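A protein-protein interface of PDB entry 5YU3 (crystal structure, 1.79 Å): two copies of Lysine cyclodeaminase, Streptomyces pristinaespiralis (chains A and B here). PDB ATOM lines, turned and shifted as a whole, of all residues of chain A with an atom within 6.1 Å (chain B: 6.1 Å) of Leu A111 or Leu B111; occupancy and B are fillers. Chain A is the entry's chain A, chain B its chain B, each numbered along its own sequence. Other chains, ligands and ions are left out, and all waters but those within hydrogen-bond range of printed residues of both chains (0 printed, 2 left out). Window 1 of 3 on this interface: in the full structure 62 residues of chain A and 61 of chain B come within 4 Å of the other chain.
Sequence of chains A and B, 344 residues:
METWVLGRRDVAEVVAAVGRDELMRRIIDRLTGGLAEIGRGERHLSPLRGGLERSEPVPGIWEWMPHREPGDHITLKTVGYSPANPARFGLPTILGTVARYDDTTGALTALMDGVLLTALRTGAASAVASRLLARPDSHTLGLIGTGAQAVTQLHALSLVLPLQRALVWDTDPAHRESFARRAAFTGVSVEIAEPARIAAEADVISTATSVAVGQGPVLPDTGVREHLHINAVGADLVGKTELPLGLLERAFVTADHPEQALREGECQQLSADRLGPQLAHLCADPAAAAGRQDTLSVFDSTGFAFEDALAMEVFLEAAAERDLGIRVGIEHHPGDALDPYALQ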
ATOM      1  N   THR A   3      -3.456  12.057   6.949  1.00  0.00           N
ATOM      2  CA  THR A   3      -4.604  11.939   7.829  1.00  0.00           C
ATOM      3  C   THR A   3      -5.330  13.274   7.908  1.00  0.00           C
ATOM      4  O   THR A   3      -4.700  14.322   8.088  1.00  0.00           O
ATOM      5  CB  THR A   3      -4.161  11.491   9.220  1.00  0.00           C
ATOM      6  OG1 THR A   3      -3.566  10.192   9.139  1.00  0.00           O
ATOM      7  CG2 THR A   3      -5.346  11.417  10.169  1.00  0.00           C
ATOM      8  N   TRP A   4      -6.651  13.234   7.780  1.00  0.00           N
ATOM      9  CA  TRP A   4      -7.481  14.420   7.969  1.00  0.00           C
ATOM     10  C   TRP A   4      -7.725  14.584   9.463  1.00  0.00           C
ATOM     11  O   TRP A   4      -8.393  13.748  10.080  1.00  0.00           O
ATOM     12  CB  TRP A   4      -8.785  14.243   7.204  1.00  0.00           C
ATOM     13  CG  TRP A   4      -9.722  15.414   7.192  1.00  0.00           C
ATOM     14  CD1 TRP A   4      -9.430  16.720   7.465  1.00  0.00           C
ATOM     15  CD2 TRP A   4     -11.115  15.366   6.872  1.00  0.00           C
ATOM     16  NE1 TRP A   4     -10.571  17.491   7.332  1.00  0.00           N
ATOM     17  CE2 TRP A   4     -11.617  16.679   6.980  1.00  0.00           C
ATOM     18  CE3 TRP A   4     -11.993  14.331   6.523  1.00  0.00           C
ATOM     19  CZ2 TRP A   4     -12.951  16.989   6.732  1.00  0.00           C
ATOM     20  CZ3 TRP A   4     -13.325  14.640   6.285  1.00  0.00           C
ATOM     21  CH2 TRP A   4     -13.788  15.962   6.387  1.00  0.00           C
ATOM     22  N   VAL A   5      -7.161  15.629  10.062  1.00  0.00           N
ATOM     23  CA  VAL A   5      -7.320  15.888  11.491  1.00  0.00           C
ATOM     24  C   VAL A   5      -8.282  17.053  11.651  1.00  0.00           C
ATOM     25  O   VAL A   5      -8.045  18.139  11.112  1.00  0.00           O
ATOM     26  CB  VAL A   5      -5.984  16.192  12.184  1.00  0.00           C
ATOM     27  CG1 VAL A   5      -6.216  16.531  13.646  1.00  0.00           C
ATOM     28  CG2 VAL A   5      -5.039  15.001  12.072  1.00  0.00           C
ATOM     29  N   LEU A   6      -9.357  16.835  12.402  1.00  0.00           N
ATOM     30  CA  LEU A   6     -10.236  17.920  12.822  1.00  0.00           C
ATOM     31  C   LEU A   6      -9.780  18.388  14.200  1.00  0.00           C
ATOM     32  O   LEU A   6      -9.976  17.685  15.192  1.00  0.00           O
ATOM     33  CB  LEU A   6     -11.688  17.455  12.850  1.00  0.00           C
ATOM     34  CG  LEU A   6     -12.323  17.036  11.527  1.00  0.00           C
ATOM     35  CD1 LEU A   6     -13.813  16.800  11.730  1.00  0.00           C
ATOM     36  CD2 LEU A   6     -12.080  18.093  10.451  1.00  0.00           C
ATOM     37  N   GLY A   7      -9.168  19.568  14.271  1.00  0.00           N
ATOM     38  CA  GLY A   7      -8.824  20.115  15.567  1.00  0.00           C
ATOM     39  C   GLY A   7     -10.061  20.472  16.372  1.00  0.00           C
ATOM     40  O   GLY A   7     -11.174  20.570  15.844  1.00  0.00           O
ATOM     41  N   THR A  97     -11.409  10.410  21.866  1.00  0.00           N
ATOM     42  CA  THR A  97     -11.149  10.773  20.477  1.00  0.00           C
ATOM     43  C   THR A  97     -11.700   9.670  19.580  1.00  0.00           C
ATOM     44  O   THR A  97     -11.869   8.528  20.010  1.00  0.00           O
ATOM     45  CB  THR A  97      -9.642  10.978  20.232  1.00  0.00           C
ATOM     46  OG1 THR A  97      -8.910  10.003  20.974  1.00  0.00           O
ATOM     47  CG2 THR A  97      -9.193  12.367  20.698  1.00  0.00           C
ATOM     48  N   VAL A  98     -11.994  10.011  18.324  1.00  0.00           N
ATOM     49  CA  VAL A  98     -12.580   9.062  17.383  1.00  0.00           C
ATOM     50  C   VAL A  98     -11.730   9.062  16.121  1.00  0.00           C
ATOM     51  O   VAL A  98     -11.481  10.125  15.541  1.00  0.00           O
ATOM     52  CB  VAL A  98     -14.045   9.393  17.032  1.00  0.00           C
ATOM     53  CG1 VAL A  98     -14.725   8.173  16.405  1.00  0.00           C
ATOM     54  CG2 VAL A  98     -14.819   9.855  18.274  1.00  0.00           C
ATOM     55  N   ALA A  99     -11.291   7.876  15.697  1.00  0.00           N
ATOM     56  CA  ALA A  99     -10.475   7.737  14.497  1.00  0.00           C
ATOM     57  C   ALA A  99     -11.204   6.909  13.446  1.00  0.00           C
ATOM     58  O   ALA A  99     -12.045   6.060  13.765  1.00  0.00           O
ATOM     59  CB  ALA A  99      -9.115   7.085  14.820  1.00  0.00           C
ATOM     60  N   ARG A 100     -10.866   7.154  12.181  1.00  0.00           N
ATOM     61  CA  ARG A 100     -11.381   6.369  11.073  1.00  0.00           C
ATOM     62  C   ARG A 100     -10.205   5.808  10.283  1.00  0.00           C
ATOM     63  O   ARG A 100      -9.212   6.509  10.065  1.00  0.00           O
ATOM     64  CB  ARG A 100     -12.277   7.215  10.162  1.00  0.00           C
ATOM     65  CG  ARG A 100     -12.895   6.417   9.032  1.00  0.00           C
ATOM     66  CD  ARG A 100     -13.984   7.197   8.333  1.00  0.00           C
ATOM     67  NE  ARG A 100     -15.180   7.294   9.163  1.00  0.00           N
ATOM     68  CZ  ARG A 100     -16.367   7.683   8.711  1.00  0.00           C
ATOM     69  NH1 ARG A 100     -16.507   8.005   7.438  1.00  0.00           N
ATOM     70  NH2 ARG A 100     -17.412   7.743   9.540  1.00  0.00           N
ATOM     71  N   LEU A 108      -4.827   5.235   8.531  1.00  0.00           N
ATOM     72  CA  LEU A 108      -5.562   6.207   9.345  1.00  0.00           C
ATOM     73  C   LEU A 108      -5.998   7.379   8.464  1.00  0.00           C
ATOM     74  O   LEU A 108      -5.157   8.145   7.991  1.00  0.00           O
ATOM     75  CB  LEU A 108      -4.678   6.682  10.496  1.00  0.00           C
ATOM     76  CG  LEU A 108      -5.202   7.833  11.356  1.00  0.00           C
ATOM     77  CD1 LEU A 108      -6.433   7.366  12.135  1.00  0.00           C
ATOM     78  CD2 LEU A 108      -4.128   8.370  12.313  1.00  0.00           C
ATOM     79  N   THR A 109      -7.308   7.530   8.232  1.00  0.00           N
ATOM     80  CA  THR A 109      -7.788   8.559   7.310  1.00  0.00           C
ATOM     81  C   THR A 109      -8.352   9.797   7.997  1.00  0.00           C
ATOM     82  O   THR A 109      -8.338  10.878   7.399  1.00  0.00           O
ATOM     83  CB  THR A 109      -8.862   8.004   6.363  1.00  0.00           C
ATOM     84  OG1 THR A 109      -9.963   7.480   7.117  1.00  0.00           O
ATOM     85  CG2 THR A 109      -8.291   6.900   5.447  1.00  0.00           C
ATOM     86  N   ALA A 110      -8.853   9.681   9.224  1.00  0.00           N
ATOM     87  CA  ALA A 110      -9.457  10.831   9.880  1.00  0.00           C
ATOM     88  C   ALA A 110      -9.400  10.650  11.390  1.00  0.00           C
ATOM     89  O   ALA A 110      -9.445   9.523  11.900  1.00  0.00           O
ATOM     90  CB  ALA A 110     -10.901  11.040   9.405  1.00  0.00           C
ATOM     91  N   LEU A 111      -9.283  11.776  12.096  1.00  0.00           N
ATOM     92  CA  LEU A 111      -9.157  11.792  13.549  1.00  0.00           C
ATOM     93  C   LEU A 111      -9.810  13.059  14.090  1.00  0.00           C
ATOM     94  O   LEU A 111      -9.547  14.144  13.569  1.00  0.00           O
ATOM     95  CB  LEU A 111      -7.675  11.744  13.951  1.00  0.00           C
ATOM     96  CG  LEU A 111      -7.358  11.906  15.433  1.00  0.00           C
ATOM     97  CD1 LEU A 111      -7.938  10.737  16.208  1.00  0.00           C
ATOM     98  CD2 LEU A 111      -5.849  11.991  15.625  1.00  0.00           C
ATOM     99  N   MET A 112     -10.630  12.934  15.141  1.00  0.00           N
ATOM    100  CA  MET A 112     -11.323  14.100  15.690  1.00  0.00           C
ATOM    101  C   MET A 112     -11.599  13.920  17.176  1.00  0.00           C
ATOM    102  O   MET A 112     -11.500  12.818  17.728  1.00  0.00           O
ATOM    103  CB  MET A 112     -12.651  14.365  14.955  1.00  0.00           C
ATOM    104  CG  MET A 112     -13.677  13.239  15.116  1.00  0.00           C
ATOM    105  SD  MET A 112     -15.293  13.648  14.413  1.00  0.00           S
ATOM    106  CE  MET A 112     -15.854  14.882  15.586  1.00  0.00           C
ATOM    107  N   ASP A 113     -11.954  15.038  17.816  1.00  0.00           N
ATOM    108  CA  ASP A 113     -12.411  15.034  19.205  1.00  0.00           C
ATOM    109  C   ASP A 113     -13.559  14.054  19.404  1.00  0.00           C
ATOM    110  O   ASP A 113     -14.429  13.902  18.539  1.00  0.00           O
ATOM    111  CB  ASP A 113     -12.893  16.435  19.599  1.00  0.00           C
ATOM    112  CG  ASP A 113     -13.642  16.439  20.919  1.00  0.00           C
ATOM    113  OD1 ASP A 113     -13.015  16.095  21.940  1.00  0.00           O
ATOM    114  OD2 ASP A 113     -14.845  16.794  20.940  1.00  0.00           O
ATOM    115  N   MET A 312     -19.755  10.671  13.866  1.00  0.00           N
ATOM    116  CA  MET A 312     -18.561  11.131  13.156  1.00  0.00           C
ATOM    117  C   MET A 312     -18.882  11.433  11.701  1.00  0.00           C
ATOM    118  O   MET A 312     -18.431  12.451  11.154  1.00  0.00           O
ATOM    119  CB  MET A 312     -17.439  10.092  13.256  1.00  0.00           C
ATOM    120  CG  MET A 312     -16.159  10.504  12.511  1.00  0.00           C
ATOM    121  SD  MET A 312     -14.706   9.663  13.187  1.00  0.00           S
ATOM    122  CE  MET A 312     -13.352  10.452  12.296  1.00  0.00           C
ATOM    123  N   ILE A 330       1.101  11.421   9.175  1.00  0.00           N
ATOM    124  CA  ILE A 330       1.489  10.745  10.409  1.00  0.00           C
ATOM    125  C   ILE A 330       2.112   9.388  10.124  1.00  0.00           C
ATOM    126  O   ILE A 330       3.229   9.108  10.559  1.00  0.00           O
ATOM    127  CB  ILE A 330       0.279  10.602  11.358  1.00  0.00           C
ATOM    128  CG1 ILE A 330      -0.378  11.969  11.615  1.00  0.00           C
ATOM    129  CG2 ILE A 330       0.709   9.947  12.682  1.00  0.00           C
ATOM    130  CD1 ILE A 330      -1.676  11.879  12.422  1.00  0.00           C
ATOM    131  N   THR B   3      -2.037  17.770  21.961  1.00  0.00           N
ATOM    132  CA  THR B   3      -1.423  16.492  21.621  1.00  0.00           C
ATOM    133  C   THR B   3      -0.121  16.711  20.862  1.00  0.00           C
ATOM    134  O   THR B   3      -0.071  17.499  19.914  1.00  0.00           O
ATOM    135  CB  THR B   3      -2.384  15.653  20.785  1.00  0.00           C
ATOM    136  OG1 THR B   3      -3.559  15.370  21.561  1.00  0.00           O
ATOM    137  CG2 THR B   3      -1.724  14.342  20.378  1.00  0.00           C
ATOM    138  N   TRP B   4       0.925  15.999  21.275  1.00  0.00           N
ATOM    139  CA  TRP B   4       2.217  16.039  20.597  1.00  0.00           C
ATOM    140  C   TRP B   4       2.192  15.027  19.457  1.00  0.00           C
ATOM    141  O   TRP B   4       2.059  13.823  19.690  1.00  0.00           O
ATOM    142  CB  TRP B   4       3.333  15.736  21.597  1.00  0.00           C
ATOM    143  CG  TRP B   4       4.726  15.824  21.058  1.00  0.00           C
ATOM    144  CD1 TRP B   4       5.145  16.479  19.931  1.00  0.00           C
ATOM    145  CD2 TRP B   4       5.889  15.228  21.635  1.00  0.00           C
ATOM    146  NE1 TRP B   4       6.508  16.327  19.777  1.00  0.00           N
ATOM    147  CE2 TRP B   4       6.985  15.563  20.812  1.00  0.00           C
ATOM    148  CE3 TRP B   4       6.112  14.446  22.773  1.00  0.00           C
ATOM    149  CZ2 TRP B   4       8.286  15.137  21.089  1.00  0.00           C
ATOM    150  CZ3 TRP B   4       7.406  14.029  23.052  1.00  0.00           C
ATOM    151  CH2 TRP B   4       8.473  14.374  22.212  1.00  0.00           C
ATOM    152  N   VAL B   5       2.279  15.511  18.222  1.00  0.00           N
ATOM    153  CA  VAL B   5       2.198  14.661  17.041  1.00  0.00           C
ATOM    154  C   VAL B   5       3.553  14.661  16.356  1.00  0.00           C
ATOM    155  O   VAL B   5       4.089  15.725  16.028  1.00  0.00           O
ATOM    156  CB  VAL B   5       1.098  15.129  16.075  1.00  0.00           C
ATOM    157  CG1 VAL B   5       1.046  14.227  14.836  1.00  0.00           C
ATOM    158  CG2 VAL B   5      -0.255  15.158  16.783  1.00  0.00           C
ATOM    159  N   LEU B   6       4.104  13.468  16.147  1.00  0.00           N
ATOM    160  CA  LEU B   6       5.303  13.304  15.334  1.00  0.00           C
ATOM    161  C   LEU B   6       4.882  13.014  13.895  1.00  0.00           C
ATOM    162  O   LEU B   6       4.217  12.010  13.630  1.00  0.00           O
ATOM    163  CB  LEU B   6       6.182  12.185  15.892  1.00  0.00           C
ATOM    164  CG  LEU B   6       6.705  12.431  17.312  1.00  0.00           C
ATOM    165  CD1 LEU B   6       7.694  11.361  17.771  1.00  0.00           C
ATOM    166  CD2 LEU B   6       7.333  13.813  17.418  1.00  0.00           C
ATOM    167  N   GLY B   7       5.245  13.902  12.971  1.00  0.00           N
ATOM    168  CA  GLY B   7       5.007  13.623  11.570  1.00  0.00           C
ATOM    169  C   GLY B   7       5.916  12.524  11.043  1.00  0.00           C
ATOM    170  O   GLY B   7       6.903  12.131  11.672  1.00  0.00           O
ATOM    171  N   THR B  97      -0.320   3.166  13.635  1.00  0.00           N
ATOM    172  CA  THR B  97      -0.016   4.370  14.391  1.00  0.00           C
ATOM    173  C   THR B  97      -0.058   4.019  15.874  1.00  0.00           C
ATOM    174  O   THR B  97      -0.718   3.064  16.288  1.00  0.00           O
ATOM    175  CB  THR B  97      -1.017   5.508  14.080  1.00  0.00           C
ATOM    176  OG1 THR B  97      -2.338   4.965  13.980  1.00  0.00           O
ATOM    177  CG2 THR B  97      -0.677   6.198  12.760  1.00  0.00           C
ATOM    178  N   VAL B  98       0.649   4.799  16.688  1.00  0.00           N
ATOM    179  CA  VAL B  98       0.733   4.539  18.120  1.00  0.00           C
ATOM    180  C   VAL B  98       0.334   5.796  18.878  1.00  0.00           C
ATOM    181  O   VAL B  98       0.911   6.866  18.658  1.00  0.00           O
ATOM    182  CB  VAL B  98       2.148   4.087  18.537  1.00  0.00           C
ATOM    183  CG1 VAL B  98       2.112   3.460  19.916  1.00  0.00           C
ATOM    184  CG2 VAL B  98       2.718   3.098  17.513  1.00  0.00           C
ATOM    185  N   ALA B  99      -0.635   5.661  19.780  1.00  0.00           N
ATOM    186  CA  ALA B  99      -1.137   6.772  20.573  1.00  0.00           C
ATOM    187  C   ALA B  99      -0.785   6.566  22.041  1.00  0.00           C
ATOM    188  O   ALA B  99      -0.724   5.434  22.526  1.00  0.00           O
ATOM    189  CB  ALA B  99      -2.659   6.912  20.409  1.00  0.00           C
ATOM    190  N   ARG B 100      -0.524   7.671  22.741  1.00  0.00           N
ATOM    191  CA  ARG B 100      -0.264   7.649  24.174  1.00  0.00           C
ATOM    192  C   ARG B 100      -1.303   8.507  24.880  1.00  0.00           C
ATOM    193  O   ARG B 100      -1.602   9.621  24.430  1.00  0.00           O
ATOM    194  CB  ARG B 100       1.149   8.148  24.494  1.00  0.00           C
ATOM    195  CG  ARG B 100       1.409   8.315  25.983  1.00  0.00           C
ATOM    196  CD  ARG B 100       2.865   8.649  26.259  1.00  0.00           C
ATOM    197  NE  ARG B 100       3.733   7.509  25.979  1.00  0.00           N
ATOM    198  CZ  ARG B 100       5.010   7.432  26.347  1.00  0.00           C
ATOM    199  NH1 ARG B 100       5.574   8.435  27.007  1.00  0.00           N
ATOM    200  NH2 ARG B 100       5.726   6.353  26.048  1.00  0.00           N
ATOM    201  N   LEU B 108      -5.339  12.388  25.501  1.00  0.00           N
ATOM    202  CA  LEU B 108      -4.435  11.991  24.425  1.00  0.00           C
ATOM    203  C   LEU B 108      -3.234  12.933  24.421  1.00  0.00           C
ATOM    204  O   LEU B 108      -3.371  14.118  24.096  1.00  0.00           O
ATOM    205  CB  LEU B 108      -5.159  12.032  23.083  1.00  0.00           C
ATOM    206  CG  LEU B 108      -4.270  11.767  21.861  1.00  0.00           C
ATOM    207  CD1 LEU B 108      -3.797  10.307  21.856  1.00  0.00           C
ATOM    208  CD2 LEU B 108      -4.991  12.099  20.559  1.00  0.00           C
ATOM    209  N   THR B 109      -2.056  12.416  24.770  1.00  0.00           N
ATOM    210  CA  THR B 109      -0.870  13.258  24.912  1.00  0.00           C
ATOM    211  C   THR B 109       0.112  13.152  23.754  1.00  0.00           C
ATOM    212  O   THR B 109       0.866  14.105  23.520  1.00  0.00           O
ATOM    213  CB  THR B 109      -0.125  12.936  26.216  1.00  0.00           C
ATOM    214  OG1 THR B 109       0.327  11.575  26.199  1.00  0.00           O
ATOM    215  CG2 THR B 109      -1.027  13.162  27.419  1.00  0.00           C
ATOM    216  N   ALA B 110       0.140  12.038  23.023  1.00  0.00           N
ATOM    217  CA  ALA B 110       1.085  11.922  21.918  1.00  0.00           C
ATOM    218  C   ALA B 110       0.583  10.925  20.885  1.00  0.00           C
ATOM    219  O   ALA B 110      -0.168   9.998  21.202  1.00  0.00           O
ATOM    220  CB  ALA B 110       2.482  11.520  22.408  1.00  0.00           C
ATOM    221  N   LEU B 111       1.017  11.127  19.638  1.00  0.00           N
ATOM    222  CA  LEU B 111       0.600  10.289  18.520  1.00  0.00           C
ATOM    223  C   LEU B 111       1.722  10.250  17.495  1.00  0.00           C
ATOM    224  O   LEU B 111       2.265  11.302  17.141  1.00  0.00           O
ATOM    225  CB  LEU B 111      -0.684  10.833  17.887  1.00  0.00           C
ATOM    226  CG  LEU B 111      -1.207  10.118  16.646  1.00  0.00           C
ATOM    227  CD1 LEU B 111      -1.672   8.705  17.006  1.00  0.00           C
ATOM    228  CD2 LEU B 111      -2.341  10.932  16.039  1.00  0.00           C
ATOM    229  N   MET B 112       2.052   9.055  16.998  1.00  0.00           N
ATOM    230  CA  MET B 112       3.142   8.938  16.031  1.00  0.00           C
ATOM    231  C   MET B 112       2.919   7.761  15.087  1.00  0.00           C
ATOM    232  O   MET B 112       2.082   6.883  15.320  1.00  0.00           O
ATOM    233  CB  MET B 112       4.497   8.785  16.738  1.00  0.00           C
ATOM    234  CG  MET B 112       4.634   7.470  17.499  1.00  0.00           C
ATOM    235  SD  MET B 112       6.286   7.233  18.197  1.00  0.00           S
ATOM    236  CE  MET B 112       7.227   7.056  16.685  1.00  0.00           C
ATOM    237  N   ASP B 113       3.696   7.761  14.003  1.00  0.00           N
ATOM    238  CA  ASP B 113       3.750   6.628  13.088  1.00  0.00           C
ATOM    239  C   ASP B 113       4.017   5.319  13.825  1.00  0.00           C
ATOM    240  O   ASP B 113       4.809   5.270  14.767  1.00  0.00           O
ATOM    241  CB  ASP B 113       4.864   6.855  12.064  1.00  0.00           C
ATOM    242  CG  ASP B 113       5.201   5.609  11.297  1.00  0.00           C
ATOM    243  OD1 ASP B 113       4.283   5.074  10.634  1.00  0.00           O
ATOM    244  OD2 ASP B 113       6.382   5.167  11.349  1.00  0.00           O
ATOM    245  N   MET B 312       8.086   3.443  21.512  1.00  0.00           N
ATOM    246  CA  MET B 312       7.607   4.820  21.429  1.00  0.00           C
ATOM    247  C   MET B 312       8.375   5.734  22.378  1.00  0.00           C
ATOM    248  O   MET B 312       8.678   6.884  22.033  1.00  0.00           O
ATOM    249  CB  MET B 312       6.112   4.872  21.734  1.00  0.00           C
ATOM    250  CG  MET B 312       5.538   6.275  21.753  1.00  0.00           C
ATOM    251  SD  MET B 312       3.792   6.215  21.326  1.00  0.00           S
ATOM    252  CE  MET B 312       3.440   7.977  21.182  1.00  0.00           C
ATOM    253  N   ILE B 330      -6.587  18.516  19.745  1.00  0.00           N
ATOM    254  CA  ILE B 330      -7.565  17.606  19.152  1.00  0.00           C
ATOM    255  C   ILE B 330      -8.773  17.425  20.058  1.00  0.00           C
ATOM    256  O   ILE B 330      -9.910  17.643  19.638  1.00  0.00           O
ATOM    257  CB  ILE B 330      -6.915  16.246  18.828  1.00  0.00           C
ATOM    258  CG1 ILE B 330      -5.710  16.429  17.901  1.00  0.00           C
ATOM    259  CG2 ILE B 330      -7.949  15.292  18.216  1.00  0.00           C
ATOM    260  CD1 ILE B 330      -4.901  15.158  17.695  1.00  0.00           C
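The backbone NH of Leu A6 is in hydrogen-bond range of the backbone carbonyl oxygen of Leu A111. N of Leu B111 sits at hydrogen-bond distance from O of Trp B4, at 2.9 Å. N of Val B98 lies within hydrogen-bond range of O of Met B112 (2.9 Å). O of Leu B111 is in hydrogen-bond range of N of Leu B6 (3.0 Å). The backbone carbonyl oxygen (O) of Trp A4 is in hydrogen-bond range of the backbone NH (N) of Leu A111.
Among the printed residues, merely in contact across the chains: Leu A111 with Leu B111 (3.7 Å), Leu A111 with Ile B330 (3.9 Å), Asp A113 with Ile B330 (3.2 Å), Ile A330 with Thr B97 (3.998 Å), Ile A330 with Leu B111 (3.8 Å), Ile A330 with Met B112 (3.9 Å) and Ile A330 with Asp B113 (3.2 Å).
Of the printed residues of chain B, Asp A113 touches Ile B330. Printed residues of chain A within 4 Å of Thr B97: Ile A330. Arg B100 touches none of the printed residues of chain A. Ala B110 touches none of the printed residues of chain A. Of the printed residues of chain A, Leu B111 touches Leu A111 and Ile A330. Printed residues of chain A within 4 Å of Asp B113: Ile A330 (3.2 Å). The nearest residue of chain A that does not touch Leu B111 is Leu A108 (4.9 Å).
Printed residues of chain B that touch a printed residue of chain A: Thr B97, Leu B111, Met B112, Asp B113 and Ile B330. Hydrophobic or aromatic side chains of chain B within 4 Å of the printed part of chain A: Leu B111 and Ile B330. Hydrophobic or aromatic side chains of chain A within 4 Å of the printed part of chain B: Leu A111 and Ile A330.
Leu B111 touches its own counterpart, Leu A111. Leu A111 touches Ile B330, and with the chains exchanged Ile A330 touches Leu B111. Asp A113 touches Ile B330, and with the chains exchanged Ile A330 touches Asp B113. Ile A330 touches Thr B97, but with the chains exchanged Thr A97 does not touch Ile B330 (4.03 Å).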
